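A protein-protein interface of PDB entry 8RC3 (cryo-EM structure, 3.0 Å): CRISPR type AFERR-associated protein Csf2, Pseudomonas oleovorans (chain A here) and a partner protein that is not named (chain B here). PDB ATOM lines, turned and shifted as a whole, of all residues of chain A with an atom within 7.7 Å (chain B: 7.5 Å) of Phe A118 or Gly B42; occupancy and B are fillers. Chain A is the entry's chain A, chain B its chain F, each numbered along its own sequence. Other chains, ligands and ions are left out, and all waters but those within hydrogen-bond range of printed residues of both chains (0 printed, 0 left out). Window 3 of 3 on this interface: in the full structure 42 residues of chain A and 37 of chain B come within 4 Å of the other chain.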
ATOM      1  N   PRO A 115     -17.133  28.494  19.816  1.00  0.00           N
ATOM      2  CA  PRO A 115     -17.032  27.188  20.475  1.00  0.00           C
ATOM      3  C   PRO A 115     -18.363  26.816  21.110  1.00  0.00           C
ATOM      4  O   PRO A 115     -18.983  27.623  21.806  1.00  0.00           O
ATOM      5  CB  PRO A 115     -15.946  27.408  21.533  1.00  0.00           C
ATOM      6  CG  PRO A 115     -16.029  28.860  21.847  1.00  0.00           C
ATOM      7  CD  PRO A 115     -16.492  29.565  20.598  1.00  0.00           C
ATOM      8  N   SER A 116     -18.802  25.588  20.863  1.00  0.00           N
ATOM      9  CA  SER A 116     -20.074  25.092  21.367  1.00  0.00           C
ATOM     10  C   SER A 116     -19.809  24.141  22.523  1.00  0.00           C
ATOM     11  O   SER A 116     -19.087  23.151  22.364  1.00  0.00           O
ATOM     12  CB  SER A 116     -20.860  24.389  20.261  1.00  0.00           C
ATOM     13  OG  SER A 116     -21.189  25.292  19.223  1.00  0.00           O
ATOM     14  N   SER A 117     -20.386  24.443  23.681  1.00  0.00           N
ATOM     15  CA  SER A 117     -20.269  23.553  24.821  1.00  0.00           C
ATOM     16  C   SER A 117     -21.152  22.327  24.621  1.00  0.00           C
ATOM     17  O   SER A 117     -22.076  22.322  23.805  1.00  0.00           O
ATOM     18  CB  SER A 117     -20.650  24.276  26.112  1.00  0.00           C
ATOM     19  OG  SER A 117     -21.971  24.775  26.040  1.00  0.00           O
ATOM     20  N   PHE A 118     -20.848  21.273  25.381  1.00  0.00           N
ATOM     21  CA  PHE A 118     -21.593  20.025  25.243  1.00  0.00           C
ATOM     22  C   PHE A 118     -23.059  20.216  25.605  1.00  0.00           C
ATOM     23  O   PHE A 118     -23.948  19.675  24.935  1.00  0.00           O
ATOM     24  CB  PHE A 118     -20.953  18.940  26.107  1.00  0.00           C
ATOM     25  CG  PHE A 118     -19.501  18.710  25.806  1.00  0.00           C
ATOM     26  CD1 PHE A 118     -19.022  18.829  24.513  1.00  0.00           C
ATOM     27  CD2 PHE A 118     -18.615  18.380  26.815  1.00  0.00           C
ATOM     28  CE1 PHE A 118     -17.688  18.621  24.234  1.00  0.00           C
ATOM     29  CE2 PHE A 118     -17.279  18.169  26.540  1.00  0.00           C
ATOM     30  CZ  PHE A 118     -16.815  18.291  25.247  1.00  0.00           C
ATOM     31  N   ASP A 119     -23.333  20.985  26.660  1.00  0.00           N
ATOM     32  CA  ASP A 119     -24.714  21.318  26.988  1.00  0.00           C
ATOM     33  C   ASP A 119     -25.372  22.097  25.858  1.00  0.00           C
ATOM     34  O   ASP A 119     -26.530  21.843  25.510  1.00  0.00           O
ATOM     35  CB  ASP A 119     -24.767  22.113  28.292  1.00  0.00           C
ATOM     36  CG  ASP A 119     -24.526  21.247  29.513  1.00  0.00           C
ATOM     37  OD1 ASP A 119     -24.865  20.046  29.467  1.00  0.00           O
ATOM     38  OD2 ASP A 119     -24.001  21.767  30.518  1.00  0.00           O
ATOM     39  N   GLU A 120     -24.646  23.050  25.271  1.00  0.00           N
ATOM     40  CA  GLU A 120     -25.188  23.803  24.145  1.00  0.00           C
ATOM     41  C   GLU A 120     -25.438  22.901  22.943  1.00  0.00           C
ATOM     42  O   GLU A 120     -26.442  23.060  22.242  1.00  0.00           O
ATOM     43  CB  GLU A 120     -24.247  24.947  23.773  1.00  0.00           C
ATOM     44  CG  GLU A 120     -24.532  26.237  24.518  1.00  0.00           C
ATOM     45  CD  GLU A 120     -23.602  27.360  24.117  1.00  0.00           C
ATOM     46  OE1 GLU A 120     -22.611  27.089  23.411  1.00  0.00           O
ATOM     47  OE2 GLU A 120     -23.865  28.516  24.505  1.00  0.00           O
ATOM     48  N   ILE A 121     -24.533  21.956  22.682  1.00  0.00           N
ATOM     49  CA  ILE A 121     -24.734  21.032  21.569  1.00  0.00           C
ATOM     50  C   ILE A 121     -25.979  20.185  21.798  1.00  0.00           C
ATOM     51  O   ILE A 121     -26.784  19.981  20.881  1.00  0.00           O
ATOM     52  CB  ILE A 121     -23.486  20.158  21.360  1.00  0.00           C
ATOM     53  CG1 ILE A 121     -22.339  20.998  20.804  1.00  0.00           C
ATOM     54  CG2 ILE A 121     -23.791  19.020  20.412  1.00  0.00           C
ATOM     55  CD1 ILE A 121     -21.091  20.205  20.516  1.00  0.00           C
ATOM     56  N   VAL A 122     -26.163  19.685  23.021  1.00  0.00           N
ATOM     57  CA  VAL A 122     -27.364  18.914  23.331  1.00  0.00           C
ATOM     58  C   VAL A 122     -28.610  19.766  23.142  1.00  0.00           C
ATOM     59  O   VAL A 122     -29.614  19.313  22.577  1.00  0.00           O
ATOM     60  CB  VAL A 122     -27.285  18.347  24.760  1.00  0.00           C
ATOM     61  CG1 VAL A 122     -28.600  17.700  25.146  1.00  0.00           C
ATOM     62  CG2 VAL A 122     -26.167  17.346  24.861  1.00  0.00           C
ATOM     63  N   THR A 123     -28.569  21.012  23.619  1.00  0.00           N
ATOM     64  CA  THR A 123     -29.735  21.886  23.544  1.00  0.00           C
ATOM     65  C   THR A 123     -30.098  22.218  22.103  1.00  0.00           C
ATOM     66  O   THR A 123     -31.279  22.214  21.737  1.00  0.00           O
ATOM     67  CB  THR A 123     -29.472  23.166  24.334  1.00  0.00           C
ATOM     68  OG1 THR A 123     -29.331  22.850  25.725  1.00  0.00           O
ATOM     69  CG2 THR A 123     -30.615  24.149  24.160  1.00  0.00           C
ATOM     70  N   MET A 124     -29.098  22.495  21.268  1.00  0.00           N
ATOM     71  CA  MET A 124     -29.350  23.031  19.938  1.00  0.00           C
ATOM     72  C   MET A 124     -29.511  21.958  18.875  1.00  0.00           C
ATOM     73  O   MET A 124     -30.280  22.153  17.928  1.00  0.00           O
ATOM     74  CB  MET A 124     -28.221  23.984  19.544  1.00  0.00           C
ATOM     75  CG  MET A 124     -28.181  25.233  20.396  1.00  0.00           C
ATOM     76  SD  MET A 124     -26.897  26.376  19.890  1.00  0.00           S
ATOM     77  CE  MET A 124     -25.462  25.513  20.501  1.00  0.00           C
ATOM     78  N   ARG A 263     -30.817  10.395  15.135  1.00  0.00           N
ATOM     79  CA  ARG A 263     -31.416  10.143  16.447  1.00  0.00           C
ATOM     80  C   ARG A 263     -32.455  11.218  16.712  1.00  0.00           C
ATOM     81  O   ARG A 263     -32.229  12.155  17.484  1.00  0.00           O
ATOM     82  CB  ARG A 263     -30.353  10.128  17.543  1.00  0.00           C
ATOM     83  CG  ARG A 263     -29.676   8.789  17.751  1.00  0.00           C
ATOM     84  CD  ARG A 263     -28.261   8.970  18.264  1.00  0.00           C
ATOM     85  NE  ARG A 263     -27.505   9.933  17.471  1.00  0.00           N
ATOM     86  CZ  ARG A 263     -27.129  11.129  17.901  1.00  0.00           C
ATOM     87  NH1 ARG A 263     -27.424  11.550  19.121  1.00  0.00           N
ATOM     88  NH2 ARG A 263     -26.443  11.925  17.088  1.00  0.00           N
ATOM     89  N   ARG B  36     -22.653   8.090  21.051  1.00  0.00           N
ATOM     90  CA  ARG B  36     -23.735   9.067  21.018  1.00  0.00           C
ATOM     91  C   ARG B  36     -25.083   8.391  21.209  1.00  0.00           C
ATOM     92  O   ARG B  36     -25.949   8.904  21.926  1.00  0.00           O
ATOM     93  CB  ARG B  36     -23.722   9.831  19.695  1.00  0.00           C
ATOM     94  CG  ARG B  36     -22.627  10.862  19.555  1.00  0.00           C
ATOM     95  CD  ARG B  36     -22.702  11.525  18.189  1.00  0.00           C
ATOM     96  NE  ARG B  36     -21.447  12.163  17.812  1.00  0.00           N
ATOM     97  CZ  ARG B  36     -20.994  13.297  18.328  1.00  0.00           C
ATOM     98  NH1 ARG B  36     -21.679  13.963  19.243  1.00  0.00           N
ATOM     99  NH2 ARG B  36     -19.826  13.778  17.913  1.00  0.00           N
ATOM    100  N   LEU B  39     -25.195   7.228  25.095  1.00  0.00           N
ATOM    101  CA  LEU B  39     -25.129   8.294  26.089  1.00  0.00           C
ATOM    102  C   LEU B  39     -25.903   9.535  25.659  1.00  0.00           C
ATOM    103  O   LEU B  39     -26.846   9.949  26.339  1.00  0.00           O
ATOM    104  CB  LEU B  39     -23.664   8.651  26.366  1.00  0.00           C
ATOM    105  CG  LEU B  39     -23.016   8.015  27.595  1.00  0.00           C
ATOM    106  CD1 LEU B  39     -22.981   6.501  27.465  1.00  0.00           C
ATOM    107  CD2 LEU B  39     -21.619   8.566  27.799  1.00  0.00           C
ATOM    108  N   GLY B  40     -25.525  10.134  24.544  1.00  0.00           N
ATOM    109  CA  GLY B  40     -26.166  11.341  24.071  1.00  0.00           C
ATOM    110  C   GLY B  40     -25.193  12.166  23.257  1.00  0.00           C
ATOM    111  O   GLY B  40     -24.104  11.717  22.913  1.00  0.00           O
ATOM    112  N   ASP B  41     -25.608  13.395  22.959  1.00  0.00           N
ATOM    113  CA  ASP B  41     -24.793  14.304  22.166  1.00  0.00           C
ATOM    114  C   ASP B  41     -23.823  15.125  23.003  1.00  0.00           C
ATOM    115  O   ASP B  41     -22.984  15.830  22.434  1.00  0.00           O
ATOM    116  CB  ASP B  41     -25.687  15.248  21.358  1.00  0.00           C
ATOM    117  CG  ASP B  41     -26.271  14.584  20.129  1.00  0.00           C
ATOM    118  OD1 ASP B  41     -25.529  13.857  19.438  1.00  0.00           O
ATOM    119  OD2 ASP B  41     -27.471  14.786  19.855  1.00  0.00           O
ATOM    120  N   GLY B  42     -23.908  15.051  24.328  1.00  0.00           N
ATOM    121  CA  GLY B  42     -23.009  15.787  25.188  1.00  0.00           C
ATOM    122  C   GLY B  42     -21.676  15.130  25.436  1.00  0.00           C
ATOM    123  O   GLY B  42     -20.859  15.665  26.191  1.00  0.00           O
ATOM    124  N   ILE B  43     -21.434  13.973  24.823  1.00  0.00           N
ATOM    125  CA  ILE B  43     -20.160  13.294  24.986  1.00  0.00           C
ATOM    126  C   ILE B  43     -19.060  14.090  24.300  1.00  0.00           C
ATOM    127  O   ILE B  43     -19.301  14.833  23.339  1.00  0.00           O
ATOM    128  CB  ILE B  43     -20.233  11.867  24.417  1.00  0.00           C
ATOM    129  CG1 ILE B  43     -20.441  11.921  22.905  1.00  0.00           C
ATOM    130  CG2 ILE B  43     -21.358  11.100  25.064  1.00  0.00           C
ATOM    131  CD1 ILE B  43     -20.152  10.627  22.204  1.00  0.00           C
ATOM    132  N   ASN B  44     -17.843  13.943  24.797  1.00  0.00           N
ATOM    133  CA  ASN B  44     -16.686  14.432  24.070  1.00  0.00           C
ATOM    134  C   ASN B  44     -16.331  13.413  22.999  1.00  0.00           C
ATOM    135  O   ASN B  44     -16.010  12.269  23.333  1.00  0.00           O
ATOM    136  CB  ASN B  44     -15.508  14.648  25.007  1.00  0.00           C
ATOM    137  CG  ASN B  44     -14.428  15.515  24.396  1.00  0.00           C
ATOM    138  OD1 ASN B  44     -14.296  15.597  23.177  1.00  0.00           O
ATOM    139  ND2 ASN B  44     -13.645  16.166  25.245  1.00  0.00           N
ATOM    140  N   PRO B  45     -16.397  13.769  21.716  1.00  0.00           N
ATOM    141  CA  PRO B  45     -16.080  12.782  20.675  1.00  0.00           C
ATOM    142  C   PRO B  45     -14.660  12.271  20.761  1.00  0.00           C
ATOM    143  O   PRO B  45     -14.390  11.140  20.339  1.00  0.00           O
ATOM    144  CB  PRO B  45     -16.327  13.555  19.373  1.00  0.00           C
ATOM    145  CG  PRO B  45     -17.169  14.722  19.762  1.00  0.00           C
ATOM    146  CD  PRO B  45     -16.756  15.075  21.147  1.00  0.00           C
ATOM    147  N   ARG B  46     -13.744  13.065  21.309  1.00  0.00           N
ATOM    148  CA  ARG B  46     -12.344  12.679  21.389  1.00  0.00           C
ATOM    149  C   ARG B  46     -12.063  11.666  22.489  1.00  0.00           C
ATOM    150  O   ARG B  46     -10.946  11.143  22.552  1.00  0.00           O
ATOM    151  CB  ARG B  46     -11.470  13.916  21.592  1.00  0.00           C
ATOM    152  CG  ARG B  46     -11.549  14.922  20.459  1.00  0.00           C
ATOM    153  CD  ARG B  46     -10.533  14.620  19.373  1.00  0.00           C
ATOM    154  NE  ARG B  46     -10.676  15.518  18.234  1.00  0.00           N
ATOM    155  CZ  ARG B  46     -10.050  16.681  18.112  1.00  0.00           C
ATOM    156  NH1 ARG B  46      -9.205  17.110  19.033  1.00  0.00           N
ATOM    157  NH2 ARG B  46     -10.277  17.430  17.038  1.00  0.00           N
ATOM    158  N   ASP B  47     -13.033  11.376  23.349  1.00  0.00           N
ATOM    159  CA  ASP B  47     -12.845  10.424  24.432  1.00  0.00           C
ATOM    160  C   ASP B  47     -13.211   9.000  24.048  1.00  0.00           C
ATOM    161  O   ASP B  47     -13.023   8.090  24.860  1.00  0.00           O
ATOM    162  CB  ASP B  47     -13.673  10.842  25.648  1.00  0.00           C
ATOM    163  CG  ASP B  47     -12.976  11.878  26.495  1.00  0.00           C
ATOM    164  OD1 ASP B  47     -11.787  12.155  26.235  1.00  0.00           O
ATOM    165  OD2 ASP B  47     -13.615  12.415  27.421  1.00  0.00           O
ATOM    166  N   HIS B  48     -13.728   8.778  22.840  1.00  0.00           N
ATOM    167  CA  HIS B  48     -14.232   7.460  22.479  1.00  0.00           C
ATOM    168  C   HIS B  48     -13.813   6.966  21.105  1.00  0.00           C
ATOM    169  O   HIS B  48     -14.020   5.783  20.825  1.00  0.00           O
ATOM    170  CB  HIS B  48     -15.764   7.447  22.550  1.00  0.00           C
ATOM    171  CG  HIS B  48     -16.311   7.887  23.871  1.00  0.00           C
ATOM    172  ND1 HIS B  48     -16.707   9.183  24.118  1.00  0.00           N
ATOM    173  CD2 HIS B  48     -16.528   7.202  25.018  1.00  0.00           C
ATOM    174  CE1 HIS B  48     -17.145   9.278  25.360  1.00  0.00           C
ATOM    175  NE2 HIS B  48     -17.047   8.090  25.928  1.00  0.00           N
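Among the printed residues, pairs that only touch across the chains: Val A122 with Gly B42 (3.3 Å), Phe A118 with Gly B42 (3.3 Å), Val A122 with Asp B41 (3.7 Å), Phe A118 with Asn B44 (3.8 Å), Ile A121 with Asp B41 (3.9 Å) and Arg A263 with Arg B36 (3.9 Å).
The guanidinium group of Arg A263 is in salt-bridge range of the side-chain carboxylate of Asp B41, 3.0 Å away.
The guanidinium group (NH1) of Arg B36 lies within salt-bridge range of the side-chain carboxylate (OD1) of Asp B41.
OD1 of Asn B44 sits close to N of Arg B46, at 3.2 Å.
The backbone carbonyl oxygen (O) of Asn B44 sits at hydrogen-bond distance from a ring nitrogen (ND1) of His B48, 3.3 Å away.
Of the 11 printed residues of chain B, 4 touch a printed residue of chain A.
Among the printed residues, Asp or Glu carboxylates within 4 Å of a Lys or Arg side-chain nitrogen of the other chain: Arg A263 with Asp B41 (3.0 Å).
Of chain B, only Gly B42 (3.3 Å) and Asn B44 (3.8 Å) come within 4 Å of Phe A118.
Gly B42 touches two residues of chain A.
Of the printed residues of chain B, Arg A263 touches Arg B36 (3.9 Å) and Asp B41 (3.0 Å).
Printed residues of chain A within 4 Å of Asn B44: Phe A118 (3.8 Å).
Of the printed residues of chain A, Arg B36 touches Arg A263 (3.9 Å).
Printed residues of chain B within 4 Å of Val A122: Asp B41 and Gly B42.
Of the printed residues of chain B, Ile A121 touches Asp B41 (3.9 Å).
The nearest residue of chain B that does not touch Phe A118 is Ile B43 (4.2 Å).
The nearest printed residue of chain B that does not touch Ile A121 is Gly B42 (5.6 Å).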
